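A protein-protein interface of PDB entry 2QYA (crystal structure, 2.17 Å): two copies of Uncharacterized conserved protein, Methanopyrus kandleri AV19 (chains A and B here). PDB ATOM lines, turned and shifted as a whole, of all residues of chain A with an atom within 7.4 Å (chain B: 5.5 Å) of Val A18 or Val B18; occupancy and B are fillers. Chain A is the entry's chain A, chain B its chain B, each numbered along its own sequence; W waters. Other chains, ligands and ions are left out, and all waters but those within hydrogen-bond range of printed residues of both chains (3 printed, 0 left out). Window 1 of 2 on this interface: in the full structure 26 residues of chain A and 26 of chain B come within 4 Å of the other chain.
Water W3 bridges OG1 of Thr A16 (2.7 Å) and ND2 of Asn B75 (3.2 Å).
Water W1 lies within hydrogen-bond range of a ring nitrogen (NE2) of His B11 (2.8 Å) and the side-chain amide oxygen of Asn A9 (2.9 Å).
Water W2 lies within hydrogen-bond range of O of Gly B12 (2.9 Å) and ND2 of Asn A9 (3.0 Å).
Hydrophobic or aromatic side chains of chain A that line the printed part of chain B: His A11, Val A18, Ala A20 and Phe A44.
Along chain B the printed residues that touch a printed residue of chain A span positions 9 to 75.
The side-chain amide nitrogen of Asn A9 lies within hydrogen-bond range of the backbone carbonyl oxygen of Phe A44 (3.5 Å).
N of Thr A71 lies within hydrogen-bond range of O of Asp A15 (2.9 Å).
The backbone NH of Leu A21 sits at hydrogen-bond distance from the backbone carbonyl oxygen of Asn A75 (2.9 Å).
The side-chain amide nitrogen of Asn A75 sits at hydrogen-bond distance from the side-chain amide oxygen of Gln A106.
N of Val B18 sits at hydrogen-bond distance from O of His B11, 3.0 Å away.
N of Val B17 lies within hydrogen-bond range of O of Thr B71 (2.8 Å).
Of chain B, only Thr B13 (3.6 Å) and Val B18 (3.9 Å) come within 4 Å of Val A18.
Printed residues of chain B within 4 Å of Asn A75: Thr B13 (3.4 Å) and Thr B16 (3.2 Å).
Of the printed residues of chain A, Thr B13 touches Asn A9, His A11, Val A18, Ala A20, Phe A44 and Asn A75.
Of the printed residues of chain A, Thr B16 touches Phe A44 (3.9 Å), Asn A75 (3.2 Å) and Gln A106 (3.4 Å).
Val B18 touches just these residues of chain A: Thr A13, Thr A16 and Val A18.
Printed residues of chain A within 4 Å of Ala B20: Gly A14 (3.9 Å).
Of the printed residues of chain A, Thr B71 touches Gln A106.
The nearest residue of chain B that does not touch Val A18 is Thr B16 (4.2 Å).
The nearest residue of chain A that does not touch Val B18 is Gly A14 (5.2 Å).
His A11 touches its own counterpart, His B11.
His A11 touches Thr B13, but with the chains exchanged Thr A13 does not touch His B11 (4.6 Å).
Thr A13 touches Asn B75, and with the chains exchanged Asn A75 touches Thr B13.
Thr A16 touches Asn B75, and with the chains exchanged Asn A75 touches Thr B16.
Among the printed residues, pairs that only touch across the chains: Asn A9 with Thr B13, His A11 with His B11, His A11 with Thr B13, Thr A13 with Asn B9, Thr A13 with Val B18, Thr A13 with Asn B75, Gly A14 with Ala B20, Gly A14 with Asn B75, Thr A16 with Val B18, Val A18 with Thr B13, Val A18 with Val B18, Ala A20 with Thr B13, Phe A44 with Gly B12, Phe A44 with Thr B13, Phe A44 with Thr B16 and Phe A44 with Val B17.
OD1 of Asn B75 lies within hydrogen-bond range of N of Asp A15.
OD1 of Asn B75 lies within hydrogen-bond range of OG1 of Thr A16.
The side-chain amide oxygen of Asn A75 sits close to the backbone carbonyl oxygen of Thr B13 (3.4 Å).
OG1 of Thr B16 is in hydrogen-bond range of ND2 of Asn A75 (3.2 Å).
OG1 of Thr B16 lies within hydrogen-bond range of OE1 of Gln A106, 3.4 Å away.
The side-chain amide oxygen of Gln A106 sits at hydrogen-bond distance from the side-chain hydroxyl of Thr B71.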
ATOM      1  N   LEU A   8      -2.710 -16.278  -3.070  1.00  0.00           N
ATOM      2  CA  LEU A   8      -2.861 -17.163  -4.221  1.00  0.00           C
ATOM      3  C   LEU A   8      -3.835 -16.541  -5.221  1.00  0.00           C
ATOM      4  O   LEU A   8      -4.985 -16.196  -4.893  1.00  0.00           O
ATOM      5  CB  LEU A   8      -3.305 -18.557  -3.802  1.00  0.00           C
ATOM      6  CG  LEU A   8      -3.552 -19.644  -4.856  1.00  0.00           C
ATOM      7  CD1 LEU A   8      -2.360 -19.919  -5.788  1.00  0.00           C
ATOM      8  CD2 LEU A   8      -3.906 -20.922  -4.135  1.00  0.00           C
ATOM      9  N   ASN A   9      -3.340 -16.379  -6.443  1.00  0.00           N
ATOM     10  CA  ASN A   9      -4.083 -15.769  -7.509  1.00  0.00           C
ATOM     11  C   ASN A   9      -4.036 -16.759  -8.657  1.00  0.00           C
ATOM     12  O   ASN A   9      -2.954 -17.012  -9.193  1.00  0.00           O
ATOM     13  CB  ASN A   9      -3.443 -14.422  -7.845  1.00  0.00           C
ATOM     14  CG  ASN A   9      -4.203 -13.638  -8.942  1.00  0.00           C
ATOM     15  OD1 ASN A   9      -5.322 -13.992  -9.331  1.00  0.00           O
ATOM     16  ND2 ASN A   9      -3.566 -12.570  -9.446  1.00  0.00           N
ATOM     17  N   ILE A  10      -5.194 -17.354  -8.977  1.00  0.00           N
ATOM     18  CA  ILE A  10      -5.369 -18.311 -10.080  1.00  0.00           C
ATOM     19  C   ILE A  10      -6.293 -17.750 -11.169  1.00  0.00           C
ATOM     20  O   ILE A  10      -7.462 -17.428 -10.899  1.00  0.00           O
ATOM     21  CB  ILE A  10      -6.011 -19.635  -9.626  1.00  0.00           C
ATOM     22  CG1 ILE A  10      -5.147 -20.358  -8.576  1.00  0.00           C
ATOM     23  CG2 ILE A  10      -6.318 -20.545 -10.857  1.00  0.00           C
ATOM     24  CD1 ILE A  10      -5.813 -21.597  -7.930  1.00  0.00           C
ATOM     25  N   HIS A  11      -5.783 -17.659 -12.393  1.00  0.00           N
ATOM     26  CA  HIS A  11      -6.571 -17.237 -13.540  1.00  0.00           C
ATOM     27  C   HIS A  11      -6.274 -18.120 -14.763  1.00  0.00           C
ATOM     28  O   HIS A  11      -5.117 -18.408 -15.064  1.00  0.00           O
ATOM     29  CB  HIS A  11      -6.278 -15.782 -13.879  1.00  0.00           C
ATOM     30  CG  HIS A  11      -7.343 -15.151 -14.703  1.00  0.00           C
ATOM     31  ND1 HIS A  11      -8.551 -14.753 -14.172  1.00  0.00           N
ATOM     32  CD2 HIS A  11      -7.417 -14.905 -16.030  1.00  0.00           C
ATOM     33  CE1 HIS A  11      -9.315 -14.265 -15.133  1.00  0.00           C
ATOM     34  NE2 HIS A  11      -8.653 -14.351 -16.272  1.00  0.00           N
ATOM     35  N   GLY A  12      -7.329 -18.562 -15.439  1.00  0.00           N
ATOM     36  CA  GLY A  12      -7.194 -19.322 -16.665  1.00  0.00           C
ATOM     37  C   GLY A  12      -7.674 -18.526 -17.870  1.00  0.00           C
ATOM     38  O   GLY A  12      -8.772 -17.961 -17.840  1.00  0.00           O
ATOM     39  N   THR A  13      -6.850 -18.488 -18.925  1.00  0.00           N
ATOM     40  CA  THR A  13      -7.216 -17.870 -20.187  1.00  0.00           C
ATOM     41  C   THR A  13      -6.539 -18.564 -21.372  1.00  0.00           C
ATOM     42  O   THR A  13      -5.383 -18.960 -21.277  1.00  0.00           O
ATOM     43  CB  THR A  13      -6.923 -16.359 -20.195  1.00  0.00           C
ATOM     44  OG1 THR A  13      -5.797 -16.077 -19.346  1.00  0.00           O
ATOM     45  CG2 THR A  13      -8.158 -15.618 -19.642  1.00  0.00           C
ATOM     46  N   GLY A  14      -7.270 -18.723 -22.477  1.00  0.00           N
ATOM     47  CA  GLY A  14      -6.753 -19.461 -23.638  1.00  0.00           C
ATOM     48  C   GLY A  14      -6.345 -20.887 -23.281  1.00  0.00           C
ATOM     49  O   GLY A  14      -7.187 -21.701 -22.873  1.00  0.00           O
ATOM     50  N   ASP A  15      -5.054 -21.187 -23.439  1.00  0.00           N
ATOM     51  CA  ASP A  15      -4.520 -22.546 -23.161  1.00  0.00           C
ATOM     52  C   ASP A  15      -3.817 -22.648 -21.829  1.00  0.00           C
ATOM     53  O   ASP A  15      -3.248 -23.704 -21.527  1.00  0.00           O
ATOM     54  CB  ASP A  15      -3.517 -22.937 -24.232  1.00  0.00           C
ATOM     55  CG  ASP A  15      -4.110 -22.932 -25.595  1.00  0.00           C
ATOM     56  OD1 ASP A  15      -4.993 -23.762 -25.844  1.00  0.00           O
ATOM     57  OD2 ASP A  15      -3.695 -22.114 -26.434  1.00  0.00           O
ATOM     58  N   THR A  16      -3.904 -21.575 -21.034  1.00  0.00           N
ATOM     59  CA  THR A  16      -2.990 -21.250 -19.928  1.00  0.00           C
ATOM     60  C   THR A  16      -3.726 -21.052 -18.574  1.00  0.00           C
ATOM     61  O   THR A  16      -4.682 -20.267 -18.478  1.00  0.00           O
ATOM     62  CB  THR A  16      -2.239 -19.914 -20.231  1.00  0.00           C
ATOM     63  OG1 THR A  16      -1.686 -19.922 -21.554  1.00  0.00           O
ATOM     64  CG2 THR A  16      -1.108 -19.666 -19.240  1.00  0.00           C
ATOM     65  N   VAL A  17      -3.276 -21.745 -17.525  1.00  0.00           N
ATOM     66  CA  VAL A  17      -3.726 -21.428 -16.156  1.00  0.00           C
ATOM     67  C   VAL A  17      -2.484 -20.963 -15.428  1.00  0.00           C
ATOM     68  O   VAL A  17      -1.466 -21.672 -15.385  1.00  0.00           O
ATOM     69  CB  VAL A  17      -4.354 -22.638 -15.423  1.00  0.00           C
ATOM     70  CG1 VAL A  17      -4.611 -22.326 -13.943  1.00  0.00           C
ATOM     71  CG2 VAL A  17      -5.631 -23.065 -16.071  1.00  0.00           C
ATOM     72  N   VAL A  18      -2.557 -19.748 -14.915  1.00  0.00           N
ATOM     73  CA  VAL A  18      -1.520 -19.197 -14.096  1.00  0.00           C
ATOM     74  C   VAL A  18      -1.904 -19.288 -12.618  1.00  0.00           C
ATOM     75  O   VAL A  18      -2.969 -18.779 -12.184  1.00  0.00           O
ATOM     76  CB  VAL A  18      -1.169 -17.728 -14.469  1.00  0.00           C
ATOM     77  CG1 VAL A  18       0.168 -17.325 -13.827  1.00  0.00           C
ATOM     78  CG2 VAL A  18      -1.016 -17.564 -15.993  1.00  0.00           C
ATOM     79  N   LEU A  19      -1.030 -19.941 -11.852  1.00  0.00           N
ATOM     80  CA  LEU A  19      -1.120 -19.967 -10.412  1.00  0.00           C
ATOM     81  C   LEU A  19       0.013 -19.101  -9.912  1.00  0.00           C
ATOM     82  O   LEU A  19       1.194 -19.440 -10.092  1.00  0.00           O
ATOM     83  CB  LEU A  19      -1.008 -21.391  -9.869  1.00  0.00           C
ATOM     84  CG  LEU A  19      -1.686 -22.568 -10.593  1.00  0.00           C
ATOM     85  CD1 LEU A  19      -1.427 -23.906  -9.900  1.00  0.00           C
ATOM     86  CD2 LEU A  19      -3.147 -22.363 -10.737  1.00  0.00           C
ATOM     87  N   ALA A  20      -0.343 -17.941  -9.356  1.00  0.00           N
ATOM     88  CA  ALA A  20       0.634 -17.022  -8.795  1.00  0.00           C
ATOM     89  C   ALA A  20       0.540 -16.971  -7.259  1.00  0.00           C
ATOM     90  O   ALA A  20      -0.542 -16.848  -6.687  1.00  0.00           O
ATOM     91  CB  ALA A  20       0.493 -15.621  -9.393  1.00  0.00           C
ATOM     92  N   LEU A  21       1.687 -17.047  -6.609  1.00  0.00           N
ATOM     93  CA  LEU A  21       1.750 -17.082  -5.156  1.00  0.00           C
ATOM     94  C   LEU A  21       2.654 -15.957  -4.766  1.00  0.00           C
ATOM     95  O   LEU A  21       3.690 -15.757  -5.401  1.00  0.00           O
ATOM     96  CB  LEU A  21       2.339 -18.402  -4.667  1.00  0.00           C
ATOM     97  CG  LEU A  21       1.504 -19.661  -4.818  1.00  0.00           C
ATOM     98  CD1 LEU A  21       2.412 -20.826  -5.156  1.00  0.00           C
ATOM     99  CD2 LEU A  21       0.771 -19.942  -3.527  1.00  0.00           C
ATOM    100  N   PHE A  44      -1.195  -7.316 -10.486  1.00  0.00           N
ATOM    101  CA  PHE A  44      -0.502  -8.579 -10.791  1.00  0.00           C
ATOM    102  C   PHE A  44      -0.407  -9.538  -9.616  1.00  0.00           C
ATOM    103  O   PHE A  44      -0.593 -10.752  -9.762  1.00  0.00           O
ATOM    104  CB  PHE A  44       0.904  -8.298 -11.302  1.00  0.00           C
ATOM    105  CG  PHE A  44       0.959  -7.995 -12.754  1.00  0.00           C
ATOM    106  CD1 PHE A  44       1.114  -9.018 -13.680  1.00  0.00           C
ATOM    107  CD2 PHE A  44       0.850  -6.686 -13.209  1.00  0.00           C
ATOM    108  CE1 PHE A  44       1.167  -8.742 -15.038  1.00  0.00           C
ATOM    109  CE2 PHE A  44       0.896  -6.393 -14.576  1.00  0.00           C
ATOM    110  CZ  PHE A  44       1.057  -7.423 -15.494  1.00  0.00           C
ATOM    111  N   THR A  71      -1.829 -25.779 -20.158  1.00  0.00           N
ATOM    112  CA  THR A  71      -0.528 -25.525 -19.550  1.00  0.00           C
ATOM    113  C   THR A  71      -0.728 -24.772 -18.226  1.00  0.00           C
ATOM    114  O   THR A  71      -1.468 -23.777 -18.183  1.00  0.00           O
ATOM    115  CB  THR A  71       0.382 -24.743 -20.496  1.00  0.00           C
ATOM    116  OG1 THR A  71       0.638 -25.568 -21.635  1.00  0.00           O
ATOM    117  CG2 THR A  71       1.725 -24.389 -19.826  1.00  0.00           C
ATOM    118  N   VAL A  72      -0.064 -25.244 -17.166  1.00  0.00           N
ATOM    119  CA  VAL A  72      -0.112 -24.596 -15.856  1.00  0.00           C
ATOM    120  C   VAL A  72       1.227 -23.900 -15.646  1.00  0.00           C
ATOM    121  O   VAL A  72       2.284 -24.555 -15.627  1.00  0.00           O
ATOM    122  CB  VAL A  72      -0.424 -25.603 -14.709  1.00  0.00           C
ATOM    123  CG1 VAL A  72      -0.304 -24.942 -13.318  1.00  0.00           C
ATOM    124  CG2 VAL A  72      -1.810 -26.233 -14.890  1.00  0.00           C
ATOM    125  N   ALA A  73       1.194 -22.566 -15.573  1.00  0.00           N
ATOM    126  CA  ALA A  73       2.381 -21.767 -15.289  1.00  0.00           C
ATOM    127  C   ALA A  73       2.294 -21.348 -13.849  1.00  0.00           C
ATOM    128  O   ALA A  73       1.251 -20.808 -13.424  1.00  0.00           O
ATOM    129  CB  ALA A  73       2.433 -20.544 -16.209  1.00  0.00           C
ATOM    130  N   ILE A  74       3.344 -21.636 -13.083  1.00  0.00           N
ATOM    131  CA  ILE A  74       3.434 -21.246 -11.670  1.00  0.00           C
ATOM    132  C   ILE A  74       4.536 -20.216 -11.486  1.00  0.00           C
ATOM    133  O   ILE A  74       5.649 -20.359 -12.006  1.00  0.00           O
ATOM    134  CB  ILE A  74       3.706 -22.461 -10.744  1.00  0.00           C
ATOM    135  CG1 ILE A  74       2.603 -23.513 -10.929  1.00  0.00           C
ATOM    136  CG2 ILE A  74       3.883 -22.021  -9.242  1.00  0.00           C
ATOM    137  CD1 ILE A  74       2.998 -24.904 -10.576  1.00  0.00           C
ATOM    138  N   ASN A  75       4.185 -19.155 -10.771  1.00  0.00           N
ATOM    139  CA  ASN A  75       5.093 -18.107 -10.394  1.00  0.00           C
ATOM    140  C   ASN A  75       4.915 -17.929  -8.885  1.00  0.00           C
ATOM    141  O   ASN A  75       3.801 -17.678  -8.428  1.00  0.00           O
ATOM    142  CB  ASN A  75       4.738 -16.788 -11.084  1.00  0.00           C
ATOM    143  CG  ASN A  75       4.023 -16.984 -12.418  1.00  0.00           C
ATOM    144  OD1 ASN A  75       2.914 -16.473 -12.605  1.00  0.00           O
ATOM    145  ND2 ASN A  75       4.648 -17.734 -13.353  1.00  0.00           N
ATOM    146  N   GLN A 106       9.723 -19.934 -11.104  1.00  0.00           N
ATOM    147  CA  GLN A 106       8.824 -19.998 -12.258  1.00  0.00           C
ATOM    148  C   GLN A 106       8.874 -21.406 -12.888  1.00  0.00           C
ATOM    149  O   GLN A 106       9.982 -21.950 -13.135  1.00  0.00           O
ATOM    150  CB  GLN A 106       9.213 -18.919 -13.257  1.00  0.00           C
ATOM    151  CG  GLN A 106       8.116 -18.570 -14.290  1.00  0.00           C
ATOM    152  CD  GLN A 106       7.987 -17.062 -14.542  1.00  0.00           C
ATOM    153  OE1 GLN A 106       6.995 -16.603 -15.097  1.00  0.00           O
ATOM    154  NE2 GLN A 106       8.985 -16.299 -14.131  1.00  0.00           N
ATOM    155  N   ASN B   9      -8.445 -11.263 -24.972  1.00  0.00           N
ATOM    156  CA  ASN B   9      -8.371 -11.316 -23.531  1.00  0.00           C
ATOM    157  C   ASN B   9      -6.920 -11.120 -23.063  1.00  0.00           C
ATOM    158  O   ASN B   9      -6.020 -11.900 -23.411  1.00  0.00           O
ATOM    159  CB  ASN B   9      -8.910 -12.666 -23.061  1.00  0.00           C
ATOM    160  CG  ASN B   9      -9.231 -12.706 -21.555  1.00  0.00           C
ATOM    161  OD1 ASN B   9      -8.626 -12.018 -20.737  1.00  0.00           O
ATOM    162  ND2 ASN B   9     -10.178 -13.548 -21.199  1.00  0.00           N
ATOM    163  N   ILE B  10      -6.687 -10.070 -22.288  1.00  0.00           N
ATOM    164  CA  ILE B  10      -5.363  -9.790 -21.742  1.00  0.00           C
ATOM    165  C   ILE B  10      -5.495  -9.822 -20.218  1.00  0.00           C
ATOM    166  O   ILE B  10      -6.302  -9.077 -19.638  1.00  0.00           O
ATOM    167  CB  ILE B  10      -4.850  -8.398 -22.207  1.00  0.00           C
ATOM    168  CG1 ILE B  10      -4.898  -8.285 -23.745  1.00  0.00           C
ATOM    169  CG2 ILE B  10      -3.454  -8.102 -21.627  1.00  0.00           C
ATOM    170  CD1 ILE B  10      -4.373  -6.969 -24.325  1.00  0.00           C
ATOM    171  N   HIS B  11      -4.738 -10.697 -19.559  1.00  0.00           N
ATOM    172  CA  HIS B  11      -4.764 -10.744 -18.099  1.00  0.00           C
ATOM    173  C   HIS B  11      -3.367 -10.942 -17.535  1.00  0.00           C
ATOM    174  O   HIS B  11      -2.630 -11.833 -17.972  1.00  0.00           O
ATOM    175  CB  HIS B  11      -5.705 -11.833 -17.608  1.00  0.00           C
ATOM    176  CG  HIS B  11      -6.144 -11.641 -16.189  1.00  0.00           C
ATOM    177  ND1 HIS B  11      -7.095 -10.711 -15.824  1.00  0.00           N
ATOM    178  CD2 HIS B  11      -5.728 -12.225 -15.038  1.00  0.00           C
ATOM    179  CE1 HIS B  11      -7.263 -10.746 -14.515  1.00  0.00           C
ATOM    180  NE2 HIS B  11      -6.444 -11.656 -14.014  1.00  0.00           N
ATOM    181  N   GLY B  12      -2.992 -10.080 -16.603  1.00  0.00           N
ATOM    182  CA  GLY B  12      -1.721 -10.165 -15.931  1.00  0.00           C
ATOM    183  C   GLY B  12      -1.962 -10.871 -14.609  1.00  0.00           C
ATOM    184  O   GLY B  12      -2.843 -10.462 -13.849  1.00  0.00           O
ATOM    185  N   THR B  13      -1.198 -11.938 -14.358  1.00  0.00           N
ATOM    186  CA  THR B  13      -1.238 -12.696 -13.100  1.00  0.00           C
ATOM    187  C   THR B  13       0.229 -12.973 -12.648  1.00  0.00           C
ATOM    188  O   THR B  13       0.927 -13.801 -13.267  1.00  0.00           O
ATOM    189  CB  THR B  13      -1.977 -14.046 -13.279  1.00  0.00           C
ATOM    190  OG1 THR B  13      -3.161 -13.886 -14.085  1.00  0.00           O
ATOM    191  CG2 THR B  13      -2.351 -14.666 -11.946  1.00  0.00           C
ATOM    192  N   THR B  16       3.341 -13.027 -15.114  1.00  0.00           N
ATOM    193  CA  THR B  16       2.959 -13.524 -16.413  1.00  0.00           C
ATOM    194  C   THR B  16       1.774 -12.731 -16.971  1.00  0.00           C
ATOM    195  O   THR B  16       0.850 -12.400 -16.237  1.00  0.00           O
ATOM    196  CB  THR B  16       2.644 -15.053 -16.298  1.00  0.00           C
ATOM    197  OG1 THR B  16       3.768 -15.728 -15.718  1.00  0.00           O
ATOM    198  CG2 THR B  16       2.365 -15.668 -17.621  1.00  0.00           C
ATOM    199  N   VAL B  17       1.844 -12.395 -18.255  1.00  0.00           N
ATOM    200  CA  VAL B  17       0.726 -11.779 -18.980  1.00  0.00           C
ATOM    201  C   VAL B  17       0.313 -12.761 -20.071  1.00  0.00           C
ATOM    202  O   VAL B  17       1.165 -13.255 -20.813  1.00  0.00           O
ATOM    203  CB  VAL B  17       1.106 -10.400 -19.608  1.00  0.00           C
ATOM    204  CG1 VAL B  17      -0.104  -9.738 -20.226  1.00  0.00           C
ATOM    205  CG2 VAL B  17       1.688  -9.474 -18.582  1.00  0.00           C
ATOM    206  N   VAL B  18      -0.983 -13.070 -20.132  1.00  0.00           N
ATOM    207  CA  VAL B  18      -1.535 -13.925 -21.163  1.00  0.00           C
ATOM    208  C   VAL B  18      -2.355 -13.051 -22.115  1.00  0.00           C
ATOM    209  O   VAL B  18      -3.249 -12.321 -21.678  1.00  0.00           O
ATOM    210  CB  VAL B  18      -2.429 -15.084 -20.596  1.00  0.00           C
ATOM    211  CG1 VAL B  18      -2.848 -16.066 -21.696  1.00  0.00           C
ATOM    212  CG2 VAL B  18      -1.712 -15.859 -19.420  1.00  0.00           C
ATOM    213  N   LEU B  19      -2.048 -13.144 -23.412  1.00  0.00           N
ATOM    214  CA  LEU B  19      -2.800 -12.468 -24.456  1.00  0.00           C
ATOM    215  C   LEU B  19      -3.478 -13.568 -25.201  1.00  0.00           C
ATOM    216  O   LEU B  19      -2.803 -14.337 -25.918  1.00  0.00           O
ATOM    217  CB  LEU B  19      -1.856 -11.690 -25.393  1.00  0.00           C
ATOM    218  CG  LEU B  19      -0.697 -10.875 -24.789  1.00  0.00           C
ATOM    219  CD1 LEU B  19       0.125 -10.175 -25.871  1.00  0.00           C
ATOM    220  CD2 LEU B  19      -1.233  -9.845 -23.838  1.00  0.00           C
ATOM    221  N   ALA B  20      -4.791 -13.696 -25.019  1.00  0.00           N
ATOM    222  CA  ALA B  20      -5.558 -14.796 -25.623  1.00  0.00           C
ATOM    223  C   ALA B  20      -6.578 -14.284 -26.656  1.00  0.00           C
ATOM    224  O   ALA B  20      -7.354 -13.340 -26.373  1.00  0.00           O
ATOM    225  CB  ALA B  20      -6.253 -15.627 -24.561  1.00  0.00           C
ATOM    226  N   THR B  71       6.716 -12.378 -18.290  1.00  0.00           N
ATOM    227  CA  THR B  71       6.585 -13.448 -19.276  1.00  0.00           C
ATOM    228  C   THR B  71       5.324 -13.129 -20.052  1.00  0.00           C
ATOM    229  O   THR B  71       4.325 -12.762 -19.458  1.00  0.00           O
ATOM    230  CB  THR B  71       6.438 -14.822 -18.597  1.00  0.00           C
ATOM    231  OG1 THR B  71       7.669 -15.172 -17.954  1.00  0.00           O
ATOM    232  CG2 THR B  71       6.080 -15.882 -19.580  1.00  0.00           C
ATOM    233  N   ALA B  73       2.622 -14.813 -22.640  1.00  0.00           N
ATOM    234  CA  ALA B  73       2.111 -15.988 -23.312  1.00  0.00           C
ATOM    235  C   ALA B  73       1.059 -15.518 -24.330  1.00  0.00           C
ATOM    236  O   ALA B  73       0.159 -14.741 -23.984  1.00  0.00           O
ATOM    237  CB  ALA B  73       1.508 -16.976 -22.312  1.00  0.00           C
ATOM    238  N   ASN B  75      -1.779 -16.963 -26.840  1.00  0.00           N
ATOM    239  CA  ASN B  75      -2.547 -18.111 -27.253  1.00  0.00           C
ATOM    240  C   ASN B  75      -3.520 -17.589 -28.298  1.00  0.00           C
ATOM    241  O   ASN B  75      -4.080 -16.496 -28.137  1.00  0.00           O
ATOM    242  CB  ASN B  75      -3.328 -18.727 -26.087  1.00  0.00           C
ATOM    243  CG  ASN B  75      -2.448 -19.124 -24.914  1.00  0.00           C
ATOM    244  OD1 ASN B  75      -2.968 -19.337 -23.812  1.00  0.00           O
ATOM    245  ND2 ASN B  75      -1.121 -19.275 -25.138  1.00  0.00           N
HETATM  246  O   HOH W   1      -6.802 -12.966 -11.585  1.00  0.00           O
HETATM  247  O   HOH W   2      -4.168 -10.257 -11.300  1.00  0.00           O
HETATM  248  O   HOH W   3       0.108 -21.313 -22.977  1.00  0.00           O
